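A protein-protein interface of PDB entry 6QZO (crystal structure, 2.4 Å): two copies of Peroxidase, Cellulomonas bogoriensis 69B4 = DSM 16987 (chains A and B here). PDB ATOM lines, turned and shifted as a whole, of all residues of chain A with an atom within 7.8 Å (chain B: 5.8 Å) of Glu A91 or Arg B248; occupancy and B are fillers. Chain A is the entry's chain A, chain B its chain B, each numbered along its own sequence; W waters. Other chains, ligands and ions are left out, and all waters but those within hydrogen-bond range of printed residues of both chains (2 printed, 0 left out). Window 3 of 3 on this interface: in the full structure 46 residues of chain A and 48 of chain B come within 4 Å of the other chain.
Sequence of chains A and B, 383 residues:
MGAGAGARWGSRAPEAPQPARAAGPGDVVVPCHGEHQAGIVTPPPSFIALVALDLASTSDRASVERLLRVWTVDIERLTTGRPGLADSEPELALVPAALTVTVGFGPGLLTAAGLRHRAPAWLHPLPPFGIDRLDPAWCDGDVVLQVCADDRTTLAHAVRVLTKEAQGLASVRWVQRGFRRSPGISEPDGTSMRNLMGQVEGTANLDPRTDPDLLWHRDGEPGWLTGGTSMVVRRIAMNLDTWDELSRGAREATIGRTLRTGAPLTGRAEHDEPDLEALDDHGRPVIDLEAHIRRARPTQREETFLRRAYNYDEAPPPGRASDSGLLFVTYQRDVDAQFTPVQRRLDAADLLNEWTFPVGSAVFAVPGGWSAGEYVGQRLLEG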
ATOM      1  N   GLY A  81     -13.240  -2.418 -19.656  1.00  0.00           N
ATOM      2  CA  GLY A  81     -13.588  -3.169 -18.438  1.00  0.00           C
ATOM      3  C   GLY A  81     -12.404  -3.973 -17.917  1.00  0.00           C
ATOM      4  O   GLY A  81     -12.630  -5.052 -17.311  1.00  0.00           O
ATOM      5  N   PRO A  83      -8.872  -3.550 -15.398  1.00  0.00           N
ATOM      6  CA  PRO A  83      -8.252  -2.671 -14.410  1.00  0.00           C
ATOM      7  C   PRO A  83      -7.174  -1.775 -15.032  1.00  0.00           C
ATOM      8  O   PRO A  83      -6.556  -2.177 -15.963  1.00  0.00           O
ATOM      9  CB  PRO A  83      -7.599  -3.629 -13.395  1.00  0.00           C
ATOM     10  CG  PRO A  83      -8.389  -4.919 -13.558  1.00  0.00           C
ATOM     11  CD  PRO A  83      -8.780  -4.970 -15.024  1.00  0.00           C
ATOM     12  N   ASP A  87      -4.138   0.486 -10.258  1.00  0.00           N
ATOM     13  CA  ASP A  87      -5.531   0.039  -9.959  1.00  0.00           C
ATOM     14  C   ASP A  87      -5.487  -1.148  -8.984  1.00  0.00           C
ATOM     15  O   ASP A  87      -5.258  -2.285  -9.400  1.00  0.00           O
ATOM     16  CB  ASP A  87      -6.311  -0.247 -11.236  1.00  0.00           C
ATOM     17  CG  ASP A  87      -7.809  -0.434 -11.022  1.00  0.00           C
ATOM     18  OD1 ASP A  87      -8.232  -0.642  -9.859  1.00  0.00           O
ATOM     19  OD2 ASP A  87      -8.538  -0.436 -12.033  1.00  0.00           O
ATOM     20  N   SER A  88      -5.721  -0.834  -7.711  1.00  0.00           N
ATOM     21  CA  SER A  88      -5.731  -1.751  -6.553  1.00  0.00           C
ATOM     22  C   SER A  88      -7.152  -2.276  -6.286  1.00  0.00           C
ATOM     23  O   SER A  88      -7.281  -3.124  -5.375  1.00  0.00           O
ATOM     24  CB  SER A  88      -5.147  -1.032  -5.352  1.00  0.00           C
ATOM     25  OG  SER A  88      -5.545   0.341  -5.332  1.00  0.00           O
ATOM     26  N   GLU A  89      -8.172  -1.824  -7.032  1.00  0.00           N
ATOM     27  CA  GLU A  89      -9.587  -2.280  -6.888  1.00  0.00           C
ATOM     28  C   GLU A  89     -10.102  -2.778  -8.237  1.00  0.00           C
ATOM     29  O   GLU A  89     -11.037  -2.229  -8.808  1.00  0.00           O
ATOM     30  CB  GLU A  89     -10.475  -1.176  -6.320  1.00  0.00           C
ATOM     31  CG  GLU A  89     -10.067  -0.716  -4.930  1.00  0.00           C
ATOM     32  CD  GLU A  89      -9.019   0.382  -4.925  1.00  0.00           C
ATOM     33  OE1 GLU A  89      -9.263   1.451  -5.549  1.00  0.00           O
ATOM     34  OE2 GLU A  89      -7.952   0.167  -4.322  1.00  0.00           O
ATOM     35  N   PRO A  90      -9.481  -3.844  -8.797  1.00  0.00           N
ATOM     36  CA  PRO A  90      -9.804  -4.298 -10.149  1.00  0.00           C
ATOM     37  C   PRO A  90     -11.285  -4.660 -10.372  1.00  0.00           C
ATOM     38  O   PRO A  90     -11.773  -4.423 -11.462  1.00  0.00           O
ATOM     39  CB  PRO A  90      -8.905  -5.533 -10.338  1.00  0.00           C
ATOM     40  CG  PRO A  90      -8.450  -5.931  -8.938  1.00  0.00           C
ATOM     41  CD  PRO A  90      -8.409  -4.636  -8.160  1.00  0.00           C
ATOM     42  N   GLU A  91     -11.952  -5.219  -9.365  1.00  0.00           N
ATOM     43  CA  GLU A  91     -13.368  -5.647  -9.463  1.00  0.00           C
ATOM     44  C   GLU A  91     -14.278  -4.440  -9.715  1.00  0.00           C
ATOM     45  O   GLU A  91     -15.375  -4.634 -10.317  1.00  0.00           O
ATOM     46  CB  GLU A  91     -13.800  -6.386  -8.198  1.00  0.00           C
ATOM     47  CG  GLU A  91     -13.211  -7.785  -8.107  1.00  0.00           C
ATOM     48  CD  GLU A  91     -11.803  -7.889  -7.547  1.00  0.00           C
ATOM     49  OE1 GLU A  91     -11.285  -6.877  -6.985  1.00  0.00           O
ATOM     50  OE2 GLU A  91     -11.217  -8.979  -7.701  1.00  0.00           O
ATOM     51  N   LEU A  92     -13.846  -3.237  -9.316  1.00  0.00           N
ATOM     52  CA  LEU A  92     -14.619  -1.994  -9.543  1.00  0.00           C
ATOM     53  C   LEU A  92     -14.482  -1.551 -11.005  1.00  0.00           C
ATOM     54  O   LEU A  92     -15.149  -0.576 -11.371  1.00  0.00           O
ATOM     55  CB  LEU A  92     -14.111  -0.897  -8.607  1.00  0.00           C
ATOM     56  CG  LEU A  92     -14.416  -1.058  -7.119  1.00  0.00           C
ATOM     57  CD1 LEU A  92     -13.991   0.176  -6.343  1.00  0.00           C
ATOM     58  CD2 LEU A  92     -15.894  -1.316  -6.882  1.00  0.00           C
ATOM     59  N   ALA A  93     -13.646  -2.224 -11.802  1.00  0.00           N
ATOM     60  CA  ALA A  93     -13.331  -1.870 -13.209  1.00  0.00           C
ATOM     61  C   ALA A  93     -14.064  -2.782 -14.195  1.00  0.00           C
ATOM     62  O   ALA A  93     -14.165  -2.408 -15.346  1.00  0.00           O
ATOM     63  CB  ALA A  93     -11.843  -1.941 -13.442  1.00  0.00           C
ATOM     64  N   LEU A  94     -14.555  -3.941 -13.759  1.00  0.00           N
ATOM     65  CA  LEU A  94     -14.972  -5.037 -14.656  1.00  0.00           C
ATOM     66  C   LEU A  94     -16.234  -4.661 -15.425  1.00  0.00           C
ATOM     67  O   LEU A  94     -16.511  -5.330 -16.441  1.00  0.00           O
ATOM     68  CB  LEU A  94     -15.179  -6.308 -13.832  1.00  0.00           C
ATOM     69  CG  LEU A  94     -13.932  -6.819 -13.125  1.00  0.00           C
ATOM     70  CD1 LEU A  94     -14.173  -8.193 -12.526  1.00  0.00           C
ATOM     71  CD2 LEU A  94     -12.736  -6.866 -14.069  1.00  0.00           C
ATOM     72  N   VAL A  95     -16.977  -3.639 -14.987  1.00  0.00           N
ATOM     73  CA  VAL A  95     -18.242  -3.211 -15.643  1.00  0.00           C
ATOM     74  C   VAL A  95     -17.980  -1.880 -16.334  1.00  0.00           C
ATOM     75  O   VAL A  95     -17.967  -0.839 -15.680  1.00  0.00           O
ATOM     76  CB  VAL A  95     -19.396  -3.131 -14.634  1.00  0.00           C
ATOM     77  CG1 VAL A  95     -20.689  -2.608 -15.262  1.00  0.00           C
ATOM     78  CG2 VAL A  95     -19.637  -4.478 -13.969  1.00  0.00           C
ATOM     79  N   THR A 153     -20.531   3.895  -9.844  1.00  0.00           N
ATOM     80  CA  THR A 153     -19.401   3.137  -9.242  1.00  0.00           C
ATOM     81  C   THR A 153     -18.272   3.043 -10.269  1.00  0.00           C
ATOM     82  O   THR A 153     -17.122   3.291  -9.893  1.00  0.00           O
ATOM     83  CB  THR A 153     -19.854   1.763  -8.735  1.00  0.00           C
ATOM     84  OG1 THR A 153     -20.856   2.006  -7.756  1.00  0.00           O
ATOM     85  CG2 THR A 153     -18.726   0.955  -8.140  1.00  0.00           C
ATOM     86  N   THR A 154     -18.599   2.701 -11.519  1.00  0.00           N
ATOM     87  CA  THR A 154     -17.651   2.690 -12.668  1.00  0.00           C
ATOM     88  C   THR A 154     -16.964   4.054 -12.773  1.00  0.00           C
ATOM     89  O   THR A 154     -15.728   4.100 -12.966  1.00  0.00           O
ATOM     90  CB  THR A 154     -18.367   2.354 -13.982  1.00  0.00           C
ATOM     91  OG1 THR A 154     -19.053   1.102 -13.851  1.00  0.00           O
ATOM     92  CG2 THR A 154     -17.412   2.284 -15.151  1.00  0.00           C
ATOM     93  N   HIS A 157     -14.676   4.841  -9.731  1.00  0.00           N
ATOM     94  CA  HIS A 157     -13.434   4.042  -9.880  1.00  0.00           C
ATOM     95  C   HIS A 157     -12.508   4.700 -10.901  1.00  0.00           C
ATOM     96  O   HIS A 157     -11.343   4.946 -10.550  1.00  0.00           O
ATOM     97  CB  HIS A 157     -13.715   2.612 -10.306  1.00  0.00           C
ATOM     98  CG  HIS A 157     -12.467   1.807 -10.319  1.00  0.00           C
ATOM     99  ND1 HIS A 157     -11.682   1.687  -9.199  1.00  0.00           N
ATOM    100  CD2 HIS A 157     -11.851   1.124 -11.296  1.00  0.00           C
ATOM    101  CE1 HIS A 157     -10.638   0.934  -9.491  1.00  0.00           C
ATOM    102  NE2 HIS A 157     -10.719   0.581 -10.770  1.00  0.00           N
ATOM    103  N   ARG B 181     -24.832   0.469  -8.007  1.00  0.00           N
ATOM    104  CA  ARG B 181     -24.860   0.344  -9.479  1.00  0.00           C
ATOM    105  C   ARG B 181     -26.236   0.808  -9.983  1.00  0.00           C
ATOM    106  O   ARG B 181     -27.173   0.930  -9.161  1.00  0.00           O
ATOM    107  CB  ARG B 181     -24.383  -1.050  -9.877  1.00  0.00           C
ATOM    108  CG  ARG B 181     -22.902  -1.242  -9.560  1.00  0.00           C
ATOM    109  CD  ARG B 181     -22.172  -2.005 -10.627  1.00  0.00           C
ATOM    110  NE  ARG B 181     -20.767  -2.252 -10.352  1.00  0.00           N
ATOM    111  CZ  ARG B 181     -19.725  -1.676 -10.965  1.00  0.00           C
ATOM    112  NH1 ARG B 181     -18.493  -2.047 -10.638  1.00  0.00           N
ATOM    113  NH2 ARG B 181     -19.901  -0.740 -11.891  1.00  0.00           N
ATOM    114  N   PRO B 188     -20.150  -7.635 -10.566  1.00  0.00           N
ATOM    115  CA  PRO B 188     -19.432  -8.835 -11.008  1.00  0.00           C
ATOM    116  C   PRO B 188     -19.823 -10.100 -10.216  1.00  0.00           C
ATOM    117  O   PRO B 188     -19.680 -10.108  -9.006  1.00  0.00           O
ATOM    118  CB  PRO B 188     -17.950  -8.471 -10.796  1.00  0.00           C
ATOM    119  CG  PRO B 188     -17.916  -6.946 -10.858  1.00  0.00           C
ATOM    120  CD  PRO B 188     -19.259  -6.486 -10.331  1.00  0.00           C
ATOM    121  N   ARG B 194     -20.924  -3.557  -4.149  1.00  0.00           N
ATOM    122  CA  ARG B 194     -19.476  -3.243  -4.126  1.00  0.00           C
ATOM    123  C   ARG B 194     -19.316  -1.857  -3.531  1.00  0.00           C
ATOM    124  O   ARG B 194     -20.040  -0.966  -3.967  1.00  0.00           O
ATOM    125  CB  ARG B 194     -18.886  -3.275  -5.535  1.00  0.00           C
ATOM    126  CG  ARG B 194     -18.678  -4.678  -6.080  1.00  0.00           C
ATOM    127  CD  ARG B 194     -17.415  -5.293  -5.542  1.00  0.00           C
ATOM    128  NE  ARG B 194     -17.261  -6.675  -6.001  1.00  0.00           N
ATOM    129  CZ  ARG B 194     -16.287  -7.474  -5.602  1.00  0.00           C
ATOM    130  NH1 ARG B 194     -15.383  -7.033  -4.746  1.00  0.00           N
ATOM    131  NH2 ARG B 194     -16.227  -8.717  -6.034  1.00  0.00           N
ATOM    132  N   GLY B 198     -13.572  -1.562  -2.722  1.00  0.00           N
ATOM    133  CA  GLY B 198     -13.589  -2.660  -3.696  1.00  0.00           C
ATOM    134  C   GLY B 198     -14.198  -3.928  -3.112  1.00  0.00           C
ATOM    135  O   GLY B 198     -14.149  -4.961  -3.796  1.00  0.00           O
ATOM    136  N   LEU B 246      -1.759  -1.353   1.298  1.00  0.00           N
ATOM    137  CA  LEU B 246      -1.951  -2.777   1.702  1.00  0.00           C
ATOM    138  C   LEU B 246      -1.946  -3.670   0.461  1.00  0.00           C
ATOM    139  O   LEU B 246      -2.642  -3.346  -0.518  1.00  0.00           O
ATOM    140  CB  LEU B 246      -3.288  -2.973   2.420  1.00  0.00           C
ATOM    141  CG  LEU B 246      -3.485  -2.288   3.765  1.00  0.00           C
ATOM    142  CD1 LEU B 246      -4.778  -2.773   4.415  1.00  0.00           C
ATOM    143  CD2 LEU B 246      -2.308  -2.527   4.707  1.00  0.00           C
ATOM    144  N   SER B 247      -1.232  -4.789   0.524  1.00  0.00           N
ATOM    145  CA  SER B 247      -1.442  -5.954  -0.372  1.00  0.00           C
ATOM    146  C   SER B 247      -2.909  -6.392  -0.321  1.00  0.00           C
ATOM    147  O   SER B 247      -3.594  -6.108   0.674  1.00  0.00           O
ATOM    148  CB  SER B 247      -0.557  -7.092   0.019  1.00  0.00           C
ATOM    149  OG  SER B 247      -1.050  -7.692   1.201  1.00  0.00           O
ATOM    150  N   ARG B 248      -3.342  -7.085  -1.362  1.00  0.00           N
ATOM    151  CA  ARG B 248      -4.632  -7.814  -1.438  1.00  0.00           C
ATOM    152  C   ARG B 248      -4.834  -8.694  -0.193  1.00  0.00           C
ATOM    153  O   ARG B 248      -5.953  -8.695   0.355  1.00  0.00           O
ATOM    154  CB  ARG B 248      -4.610  -8.694  -2.687  1.00  0.00           C
ATOM    155  CG  ARG B 248      -5.979  -9.066  -3.215  1.00  0.00           C
ATOM    156  CD  ARG B 248      -6.420  -8.174  -4.358  1.00  0.00           C
ATOM    157  NE  ARG B 248      -7.430  -8.944  -5.078  1.00  0.00           N
ATOM    158  CZ  ARG B 248      -8.514  -8.450  -5.653  1.00  0.00           C
ATOM    159  NH1 ARG B 248      -9.344  -9.282  -6.244  1.00  0.00           N
ATOM    160  NH2 ARG B 248      -8.743  -7.152  -5.690  1.00  0.00           N
ATOM    161  N   GLY B 249      -3.804  -9.446   0.208  1.00  0.00           N
ATOM    162  CA  GLY B 249      -3.857 -10.398   1.335  1.00  0.00           C
ATOM    163  C   GLY B 249      -4.168  -9.703   2.650  1.00  0.00           C
ATOM    164  O   GLY B 249      -4.983 -10.245   3.438  1.00  0.00           O
ATOM    165  N   ALA B 250      -3.535  -8.554   2.882  1.00  0.00           N
ATOM    166  CA  ALA B 250      -3.711  -7.718   4.094  1.00  0.00           C
ATOM    167  C   ALA B 250      -5.116  -7.100   4.102  1.00  0.00           C
ATOM    168  O   ALA B 250      -5.684  -6.970   5.203  1.00  0.00           O
ATOM    169  CB  ALA B 250      -2.632  -6.657   4.171  1.00  0.00           C
ATOM    170  N   ARG B 251      -5.656  -6.738   2.934  1.00  0.00           N
ATOM    171  CA  ARG B 251      -7.020  -6.160   2.813  1.00  0.00           C
ATOM    172  C   ARG B 251      -8.067  -7.223   3.118  1.00  0.00           C
ATOM    173  O   ARG B 251      -9.095  -6.902   3.740  1.00  0.00           O
ATOM    174  CB  ARG B 251      -7.294  -5.648   1.399  1.00  0.00           C
ATOM    175  CG  ARG B 251      -6.543  -4.374   1.031  1.00  0.00           C
ATOM    176  CD  ARG B 251      -6.866  -3.959  -0.387  1.00  0.00           C
ATOM    177  NE  ARG B 251      -6.364  -2.632  -0.676  1.00  0.00           N
ATOM    178  CZ  ARG B 251      -6.621  -1.944  -1.787  1.00  0.00           C
ATOM    179  NH1 ARG B 251      -7.382  -2.470  -2.735  1.00  0.00           N
ATOM    180  NH2 ARG B 251      -6.114  -0.728  -1.945  1.00  0.00           N
ATOM    181  N   GLU B 252      -7.836  -8.444   2.647  1.00  0.00           N
ATOM    182  CA  GLU B 252      -8.752  -9.587   2.852  1.00  0.00           C
ATOM    183  C   GLU B 252      -8.694  -9.997   4.322  1.00  0.00           C
ATOM    184  O   GLU B 252      -9.764 -10.243   4.903  1.00  0.00           O
ATOM    185  CB  GLU B 252      -8.391 -10.691   1.873  1.00  0.00           C
ATOM    186  CG  GLU B 252      -8.745 -10.331   0.438  1.00  0.00           C
ATOM    187  CD  GLU B 252      -8.426 -11.377  -0.603  1.00  0.00           C
ATOM    188  OE1 GLU B 252      -7.551 -12.222  -0.325  1.00  0.00           O
ATOM    189  OE2 GLU B 252      -9.076 -11.356  -1.669  1.00  0.00           O
ATOM    190  N   ALA B 253      -7.504 -10.020   4.920  1.00  0.00           N
ATOM    191  CA  ALA B 253      -7.314 -10.364   6.346  1.00  0.00           C
ATOM    192  C   ALA B 253      -8.080  -9.350   7.219  1.00  0.00           C
ATOM    193  O   ALA B 253      -8.634  -9.762   8.240  1.00  0.00           O
ATOM    194  CB  ALA B 253      -5.850 -10.419   6.697  1.00  0.00           C
ATOM    195  N   LEU B 259     -11.749 -10.410  -1.886  1.00  0.00           N
ATOM    196  CA  LEU B 259     -12.272  -9.265  -2.679  1.00  0.00           C
ATOM    197  C   LEU B 259     -12.926  -9.797  -3.962  1.00  0.00           C
ATOM    198  O   LEU B 259     -13.978  -9.250  -4.356  1.00  0.00           O
ATOM    199  CB  LEU B 259     -11.136  -8.283  -2.944  1.00  0.00           C
ATOM    200  CG  LEU B 259     -10.703  -7.512  -1.699  1.00  0.00           C
ATOM    201  CD1 LEU B 259      -9.294  -6.959  -1.817  1.00  0.00           C
ATOM    202  CD2 LEU B 259     -11.682  -6.397  -1.415  1.00  0.00           C
ATOM    203  N   ARG B 260     -12.377 -10.855  -4.541  1.00  0.00           N
ATOM    204  CA  ARG B 260     -12.847 -11.381  -5.846  1.00  0.00           C
ATOM    205  C   ARG B 260     -14.264 -11.935  -5.674  1.00  0.00           C
ATOM    206  O   ARG B 260     -15.189 -11.337  -6.207  1.00  0.00           O
ATOM    207  CB  ARG B 260     -11.876 -12.416  -6.428  1.00  0.00           C
ATOM    208  CG  ARG B 260     -12.147 -12.671  -7.905  1.00  0.00           C
ATOM    209  CD  ARG B 260     -11.498 -13.871  -8.539  1.00  0.00           C
ATOM    210  NE  ARG B 260     -12.619 -14.650  -9.040  1.00  0.00           N
ATOM    211  CZ  ARG B 260     -12.816 -15.948  -8.826  1.00  0.00           C
ATOM    212  NH1 ARG B 260     -11.925 -16.672  -8.151  1.00  0.00           N
ATOM    213  NH2 ARG B 260     -13.918 -16.513  -9.305  1.00  0.00           N
HETATM  214  O   HOH W   1      -9.931  -3.921  -3.343  1.00  0.00           O
HETATM  215  O   HOH W   2     -11.632  -4.846  -5.140  1.00  0.00           O
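The side-chain carboxylate (OE2) of Glu A89 is in salt-bridge range of the guanidinium group (NH1) of Arg B251 (3.1 Å).
The side-chain carboxylate (OE1) of Glu A91 is in salt-bridge range of the guanidinium group (NH2) of Arg B248 (2.9 Å).
OG1 of Thr A154 sits at hydrogen-bond distance from NH2 of Arg B181, at 2.8 Å.
The backbone carbonyl oxygen (O) of Ser A88 lies within hydrogen-bond range of the guanidinium group (NH1) of Arg B251, at 2.7 Å.
The backbone carbonyl oxygen of Arg B260 lies within hydrogen-bond range of the guanidinium group of Arg B194 (2.8 Å).
The side-chain carboxylate (OD1) of Asp A87 sits at hydrogen-bond distance from the backbone NH (N) of Glu A89.
NE2 of His A157 lies close to O of Glu A89, at 3.4 Å.
O of Leu B259 is in hydrogen-bond range of NH1 of Arg B194 (2.7 Å).
The guanidinium group of Arg B194 lies within hydrogen-bond range of the backbone carbonyl oxygen of Gly B198.
O of Val A95 is in hydrogen-bond range of OG1 of Thr A154 (2.9 Å).
Pro A90 touches Arg B248.
Glu A91 touches Pro B188 (O to CG, 3.5 Å).
CB of Glu A91 touches CZ of Arg B194, 3.8 Å away.
OE2 of Glu A91 touches CA of Arg B260, at 3.4 Å.
Leu A92 touches Arg B181 (O to NH1, 3.7 Å).
Leu A92 touches Arg B194.
Leu A92 touches Gly B198.
CB of Val A95 touches NH2 of Arg B181 (3.7 Å).
Thr A153 touches Arg B181 (CG2 to NH1, 3.9 Å).
Of the printed residues of chain B, Glu A89 touches Arg B251.
Of chain B, only Pro B188 (3.5 Å), Arg B194 (3.8 Å), Arg B248 (2.4 Å) and Arg B260 (3.4 Å) come within 4 Å of Glu A91.
Of the printed residues of chain B, Val A95 touches Arg B181 (3.7 Å).
Printed residues of chain A within 4 Å of Arg B181: Leu A92 (3.7 Å), Val A95 (3.7 Å), Thr A153 (3.9 Å) and Thr A154 (2.8 Å).
Of the printed residues of chain A, Gly B198 touches Leu A92.
No residue of chain A comes within 4 Å of Ser B247.
Arg B248 touches just these residues of chain A: Pro A90 (3.5 Å) and Glu A91 (2.4 Å).
No residue of chain A comes within 4 Å of Gly B249.
Printed residues of chain A within 4 Å of Arg B251: Ser A88 and Glu A89.
Leu B259 touches none of the printed residues of chain A.
Of the 14 printed residues of chain B, 7 touch a printed residue of chain A.
Printed residues of chain B that touch a printed residue of chain A: Arg B181, Pro B188, Arg B194, Gly B198, Arg B248, Arg B251 and Arg B260.
Hydrophobic or aromatic side chains of chain B within 4 Å of the printed part of chain A: Pro B188.
Along chain B the printed residues that touch a printed residue of chain A span positions 181 to 260.
Among the printed residues, 13 pairs touch across the chains.
No position is printed for both chains.
Of the 13 pairs that touch across the chains among the printed residues, none has its exchanged pair printed and touching as well.
Water W2 bridges the side-chain carboxylate of Glu A91 and the backbone carbonyl oxygen of Gly B198.
Water W1 lies within hydrogen-bond range of NH1 of Arg B251 and O of Ser A88.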
